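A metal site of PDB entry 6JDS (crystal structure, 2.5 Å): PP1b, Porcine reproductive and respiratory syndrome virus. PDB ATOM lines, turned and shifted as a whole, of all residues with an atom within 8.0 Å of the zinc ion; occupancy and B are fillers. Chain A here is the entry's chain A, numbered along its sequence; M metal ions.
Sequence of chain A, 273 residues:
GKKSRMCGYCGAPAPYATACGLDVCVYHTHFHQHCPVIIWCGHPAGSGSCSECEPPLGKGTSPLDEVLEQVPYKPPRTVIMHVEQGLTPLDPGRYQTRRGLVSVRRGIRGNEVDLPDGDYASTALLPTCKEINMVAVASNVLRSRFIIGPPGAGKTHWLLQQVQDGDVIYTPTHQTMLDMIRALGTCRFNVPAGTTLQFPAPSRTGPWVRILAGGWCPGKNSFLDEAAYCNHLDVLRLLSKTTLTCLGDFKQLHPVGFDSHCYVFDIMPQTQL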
ATOM      1  N   TYR A   9     -19.042   4.630 -13.070  1.00  0.00           N
ATOM      2  CA  TYR A   9     -19.322   5.571 -11.994  1.00  0.00           C
ATOM      3  C   TYR A   9     -18.937   7.007 -12.385  1.00  0.00           C
ATOM      4  O   TYR A   9     -19.773   7.901 -12.365  1.00  0.00           O
ATOM      5  CB  TYR A   9     -18.558   5.197 -10.727  1.00  0.00           C
ATOM      6  CG  TYR A   9     -19.045   3.946 -10.021  1.00  0.00           C
ATOM      7  CD1 TYR A   9     -20.251   3.942  -9.330  1.00  0.00           C
ATOM      8  CD2 TYR A   9     -18.273   2.777 -10.022  1.00  0.00           C
ATOM      9  CE1 TYR A   9     -20.686   2.803  -8.669  1.00  0.00           C
ATOM     10  CE2 TYR A   9     -18.712   1.644  -9.367  1.00  0.00           C
ATOM     11  CZ  TYR A   9     -19.918   1.657  -8.690  1.00  0.00           C
ATOM     12  OH  TYR A   9     -20.357   0.525  -8.034  1.00  0.00           O
ATOM     13  N   ALA A  17     -13.204  -4.356 -14.790  1.00  0.00           N
ATOM     14  CA  ALA A  17     -14.650  -4.525 -14.812  1.00  0.00           C
ATOM     15  C   ALA A  17     -15.117  -5.361 -13.637  1.00  0.00           C
ATOM     16  O   ALA A  17     -14.370  -6.176 -13.088  1.00  0.00           O
ATOM     17  CB  ALA A  17     -15.083  -5.174 -16.116  1.00  0.00           C
ATOM     18  N   THR A  18     -16.371  -5.152 -13.240  1.00  0.00           N
ATOM     19  CA  THR A  18     -16.980  -5.918 -12.166  1.00  0.00           C
ATOM     20  C   THR A  18     -17.423  -7.247 -12.746  1.00  0.00           C
ATOM     21  O   THR A  18     -17.562  -7.385 -13.969  1.00  0.00           O
ATOM     22  CB  THR A  18     -18.198  -5.206 -11.562  1.00  0.00           C
ATOM     23  OG1 THR A  18     -19.206  -5.038 -12.568  1.00  0.00           O
ATOM     24  CG2 THR A  18     -17.805  -3.849 -10.999  1.00  0.00           C
ATOM     25  N   ALA A  19     -17.662  -8.219 -11.869  1.00  0.00           N
ATOM     26  CA  ALA A  19     -18.198  -9.508 -12.287  1.00  0.00           C
ATOM     27  C   ALA A  19     -19.586  -9.354 -12.921  1.00  0.00           C
ATOM     28  O   ALA A  19     -19.992 -10.180 -13.745  1.00  0.00           O
ATOM     29  CB  ALA A  19     -18.254 -10.468 -11.112  1.00  0.00           C
ATOM     30  N   CYS A  20     -20.311  -8.302 -12.536  1.00  0.00           N
ATOM     31  CA  CYS A  20     -21.665  -8.029 -13.029  1.00  0.00           C
ATOM     32  C   CYS A  20     -21.727  -7.109 -14.265  1.00  0.00           C
ATOM     33  O   CYS A  20     -22.817  -6.709 -14.669  1.00  0.00           O
ATOM     34  CB  CYS A  20     -22.508  -7.451 -11.892  1.00  0.00           C
ATOM     35  SG  CYS A  20     -22.079  -5.760 -11.412  1.00  0.00           S
ATOM     36  N   GLY A  21     -20.575  -6.773 -14.843  1.00  0.00           N
ATOM     37  CA  GLY A  21     -20.533  -6.101 -16.150  1.00  0.00           C
ATOM     38  C   GLY A  21     -20.302  -4.592 -16.182  1.00  0.00           C
ATOM     39  O   GLY A  21     -20.377  -3.992 -17.254  1.00  0.00           O
ATOM     40  N   LEU A  22     -20.015  -3.990 -15.027  1.00  0.00           N
ATOM     41  CA  LEU A  22     -19.731  -2.556 -14.966  1.00  0.00           C
ATOM     42  C   LEU A  22     -18.240  -2.299 -15.125  1.00  0.00           C
ATOM     43  O   LEU A  22     -17.426  -2.926 -14.447  1.00  0.00           O
ATOM     44  CB  LEU A  22     -20.197  -1.973 -13.627  1.00  0.00           C
ATOM     45  CG  LEU A  22     -20.203  -0.453 -13.495  1.00  0.00           C
ATOM     46  CD1 LEU A  22     -21.400   0.162 -14.214  1.00  0.00           C
ATOM     47  CD2 LEU A  22     -20.205  -0.027 -12.031  1.00  0.00           C
ATOM     48  N   HIS A  32     -17.083  -1.285  -4.862  1.00  0.00           N
ATOM     49  CA  HIS A  32     -18.151  -2.067  -5.462  1.00  0.00           C
ATOM     50  C   HIS A  32     -18.397  -3.327  -4.639  1.00  0.00           C
ATOM     51  O   HIS A  32     -17.892  -4.402  -4.959  1.00  0.00           O
ATOM     52  CB  HIS A  32     -17.803  -2.413  -6.916  1.00  0.00           C
ATOM     53  CG  HIS A  32     -18.948  -2.956  -7.693  1.00  0.00           C
ATOM     54  ND1 HIS A  32     -19.918  -2.146  -8.255  1.00  0.00           N
ATOM     55  CD2 HIS A  32     -19.293  -4.226  -8.010  1.00  0.00           C
ATOM     56  CE1 HIS A  32     -20.805  -2.896  -8.882  1.00  0.00           C
ATOM     57  NE2 HIS A  32     -20.451  -4.164  -8.746  1.00  0.00           N
ATOM     58  N   GLN A  33     -19.183  -3.170  -3.583  1.00  0.00           N
ATOM     59  CA  GLN A  33     -19.474  -4.235  -2.625  1.00  0.00           C
ATOM     60  C   GLN A  33     -20.305  -5.364  -3.251  1.00  0.00           C
ATOM     61  O   GLN A  33     -20.219  -6.505  -2.813  1.00  0.00           O
ATOM     62  CB  GLN A  33     -20.236  -3.679  -1.421  1.00  0.00           C
ATOM     63  CG  GLN A  33     -19.482  -2.633  -0.599  1.00  0.00           C
ATOM     64  CD  GLN A  33     -18.527  -3.227   0.433  1.00  0.00           C
ATOM     65  OE1 GLN A  33     -17.460  -2.661   0.691  1.00  0.00           O
ATOM     66  NE2 GLN A  33     -18.905  -4.355   1.017  1.00  0.00           N
ATOM     67  N   HIS A  34     -21.120  -5.024  -4.253  1.00  0.00           N
ATOM     68  CA  HIS A  34     -22.057  -5.958  -4.868  1.00  0.00           C
ATOM     69  C   HIS A  34     -21.434  -7.284  -5.305  1.00  0.00           C
ATOM     70  O   HIS A  34     -21.988  -8.349  -5.042  1.00  0.00           O
ATOM     71  CB  HIS A  34     -22.749  -5.280  -6.060  1.00  0.00           C
ATOM     72  CG  HIS A  34     -23.596  -6.212  -6.871  1.00  0.00           C
ATOM     73  ND1 HIS A  34     -23.369  -6.431  -8.212  1.00  0.00           N
ATOM     74  CD2 HIS A  34     -24.652  -6.992  -6.543  1.00  0.00           C
ATOM     75  CE1 HIS A  34     -24.253  -7.286  -8.677  1.00  0.00           C
ATOM     76  NE2 HIS A  34     -25.047  -7.647  -7.683  1.00  0.00           N
ATOM     77  N   CYS A  35     -20.286  -7.213  -5.980  1.00  0.00           N
ATOM     78  CA  CYS A  35     -19.670  -8.415  -6.556  1.00  0.00           C
ATOM     79  C   CYS A  35     -18.154  -8.235  -6.702  1.00  0.00           C
ATOM     80  O   CYS A  35     -17.652  -7.101  -6.602  1.00  0.00           O
ATOM     81  CB  CYS A  35     -20.300  -8.722  -7.917  1.00  0.00           C
ATOM     82  SG  CYS A  35     -19.783  -7.620  -9.247  1.00  0.00           S
ATOM     83  N   PRO A  36     -17.409  -9.336  -6.942  1.00  0.00           N
ATOM     84  CA  PRO A  36     -15.946  -9.244  -7.049  1.00  0.00           C
ATOM     85  C   PRO A  36     -15.449  -8.396  -8.217  1.00  0.00           C
ATOM     86  O   PRO A  36     -16.097  -8.329  -9.261  1.00  0.00           O
ATOM     87  CB  PRO A  36     -15.514 -10.703  -7.251  1.00  0.00           C
ATOM     88  CG  PRO A  36     -16.647 -11.523  -6.747  1.00  0.00           C
ATOM     89  CD  PRO A  36     -17.879 -10.725  -7.052  1.00  0.00           C
ATOM     90  N   VAL A  37     -14.297  -7.749  -8.012  1.00  0.00           N
ATOM     91  CA  VAL A  37     -13.622  -6.991  -9.058  1.00  0.00           C
ATOM     92  C   VAL A  37     -12.179  -7.467  -9.125  1.00  0.00           C
ATOM     93  O   VAL A  37     -11.396  -7.223  -8.209  1.00  0.00           O
ATOM     94  CB  VAL A  37     -13.660  -5.474  -8.772  1.00  0.00           C
ATOM     95  CG1 VAL A  37     -12.975  -4.701  -9.892  1.00  0.00           C
ATOM     96  CG2 VAL A  37     -15.088  -5.000  -8.585  1.00  0.00           C
ATOM     97  N   ASP A  65     -25.243   1.692  -6.513  1.00  0.00           N
ATOM     98  CA  ASP A  65     -24.891   0.774  -5.432  1.00  0.00           C
ATOM     99  C   ASP A  65     -26.103   0.442  -4.556  1.00  0.00           C
ATOM    100  O   ASP A  65     -26.252  -0.696  -4.115  1.00  0.00           O
ATOM    101  CB  ASP A  65     -23.751   1.342  -4.573  1.00  0.00           C
ATOM    102  CG  ASP A  65     -22.478   1.550  -5.366  1.00  0.00           C
ATOM    103  OD1 ASP A  65     -21.979   0.573  -5.972  1.00  0.00           O
ATOM    104  OD2 ASP A  65     -21.958   2.684  -5.394  1.00  0.00           O
ATOM    105  N   LEU A  68     -28.171  -2.025  -6.506  1.00  0.00           N
ATOM    106  CA  LEU A  68     -27.532  -3.343  -6.496  1.00  0.00           C
ATOM    107  C   LEU A  68     -27.665  -4.108  -5.179  1.00  0.00           C
ATOM    108  O   LEU A  68     -27.449  -5.312  -5.138  1.00  0.00           O
ATOM    109  CB  LEU A  68     -26.056  -3.228  -6.904  1.00  0.00           C
ATOM    110  CG  LEU A  68     -25.824  -2.947  -8.387  1.00  0.00           C
ATOM    111  CD1 LEU A  68     -24.371  -2.553  -8.648  1.00  0.00           C
ATOM    112  CD2 LEU A  68     -26.226  -4.129  -9.247  1.00  0.00           C
ATOM    113  N   VAL A  71     -30.191  -6.673  -5.745  1.00  0.00           N
ATOM    114  CA  VAL A  71     -29.864  -7.601  -6.839  1.00  0.00           C
ATOM    115  C   VAL A  71     -28.664  -8.462  -6.449  1.00  0.00           C
ATOM    116  O   VAL A  71     -27.525  -8.114  -6.754  1.00  0.00           O
ATOM    117  CB  VAL A  71     -29.566  -6.830  -8.151  1.00  0.00           C
ATOM    118  CG1 VAL A  71     -29.321  -7.806  -9.308  1.00  0.00           C
ATOM    119  CG2 VAL A  71     -30.696  -5.871  -8.481  1.00  0.00           C
ATOM    120  N   PRO A  72     -28.918  -9.592  -5.757  1.00  0.00           N
ATOM    121  CA  PRO A  72     -27.812 -10.444  -5.272  1.00  0.00           C
ATOM    122  C   PRO A  72     -26.970 -11.040  -6.394  1.00  0.00           C
ATOM    123  O   PRO A  72     -27.517 -11.565  -7.362  1.00  0.00           O
ATOM    124  CB  PRO A  72     -28.538 -11.548  -4.497  1.00  0.00           C
ATOM    125  CG  PRO A  72     -29.879 -10.997  -4.167  1.00  0.00           C
ATOM    126  CD  PRO A  72     -30.222 -10.110  -5.325  1.00  0.00           C
ATOM    127  N   TYR A  73     -25.652 -10.949  -6.250  1.00  0.00           N
ATOM    128  CA  TYR A  73     -24.731 -11.483  -7.243  1.00  0.00           C
ATOM    129  C   TYR A  73     -24.736 -13.011  -7.243  1.00  0.00           C
ATOM    130  O   TYR A  73     -24.491 -13.636  -6.205  1.00  0.00           O
ATOM    131  CB  TYR A  73     -23.305 -10.959  -7.006  1.00  0.00           C
ATOM    132  CG  TYR A  73     -22.274 -11.617  -7.899  1.00  0.00           C
ATOM    133  CD1 TYR A  73     -22.336 -11.478  -9.282  1.00  0.00           C
ATOM    134  CD2 TYR A  73     -21.242 -12.375  -7.357  1.00  0.00           C
ATOM    135  CE1 TYR A  73     -21.404 -12.078 -10.106  1.00  0.00           C
ATOM    136  CE2 TYR A  73     -20.306 -12.981  -8.174  1.00  0.00           C
ATOM    137  CZ  TYR A  73     -20.383 -12.827  -9.546  1.00  0.00           C
ATOM    138  OH  TYR A  73     -19.448 -13.428 -10.356  1.00  0.00           O
ATOM    139  N   LEU A 126     -21.638 -10.988 -16.078  1.00  0.00           N
ATOM    140  CA  LEU A 126     -23.086 -10.933 -16.165  1.00  0.00           C
ATOM    141  C   LEU A 126     -23.501  -9.636 -16.875  1.00  0.00           C
ATOM    142  O   LEU A 126     -22.724  -8.687 -16.912  1.00  0.00           O
ATOM    143  CB  LEU A 126     -23.721 -11.004 -14.775  1.00  0.00           C
ATOM    144  CG  LEU A 126     -23.341 -12.227 -13.923  1.00  0.00           C
ATOM    145  CD1 LEU A 126     -24.041 -12.173 -12.578  1.00  0.00           C
ATOM    146  CD2 LEU A 126     -23.670 -13.529 -14.637  1.00  0.00           C
ATOM    147  N   THR A 128     -25.826  -7.672 -15.852  1.00  0.00           N
ATOM    148  CA  THR A 128     -26.473  -6.842 -14.840  1.00  0.00           C
ATOM    149  C   THR A 128     -26.234  -5.342 -15.005  1.00  0.00           C
ATOM    150  O   THR A 128     -27.181  -4.572 -15.029  1.00  0.00           O
ATOM    151  CB  THR A 128     -26.017  -7.253 -13.429  1.00  0.00           C
ATOM    152  OG1 THR A 128     -26.062  -8.683 -13.306  1.00  0.00           O
ATOM    153  CG2 THR A 128     -26.889  -6.634 -12.342  1.00  0.00           C
ATOM    154  N   CYS A 129     -24.967  -4.936 -15.120  1.00  0.00           N
ATOM    155  CA  CYS A 129     -24.606  -3.521 -15.253  1.00  0.00           C
ATOM    156  C   CYS A 129     -23.947  -3.206 -16.602  1.00  0.00           C
ATOM    157  O   CYS A 129     -23.153  -2.279 -16.709  1.00  0.00           O
ATOM    158  CB  CYS A 129     -23.683  -3.097 -14.101  1.00  0.00           C
ATOM    159  SG  CYS A 129     -24.502  -3.050 -12.497  1.00  0.00           S
HETATM  160 ZN    ZN M   1     -21.465  -6.114  -9.265  1.00  0.00          ZN
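The side-chain hydroxyl (OH) of Tyr 9 sits at hydrogen-bond distance from a ring nitrogen (ND1) of His 32 (2.7 Å). The backbone NH of Thr 128 sits at hydrogen-bond distance from the backbone carbonyl oxygen of Cys 20, at 3.4 Å. N of Ala 19 sits close to SG of Cys 35 (3.4 Å). O of Cys 20 is in hydrogen-bond range of N of Cys 129 (2.8 Å). N of Cys 20 sits close to OG1 of Thr 18 (3.4 Å). The backbone carbonyl oxygen (O) of Val 71 lies within hydrogen-bond range of a ring nitrogen (NE2) of His 34.
Of the 21 residues printed, 4 come within 4 Å of the zinc ion.
ND1 of His 34 is bound to the zinc ion (2.2 Å). SG of Cys 35 is bound to the zinc ion. The zinc ion is bound by NE2 of His 32 (2.3 Å). The zinc ion is bound by the side-chain sulfur (SG) of Cys 20 (2.3 Å). The zinc ion has four donor atoms within binding distance.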
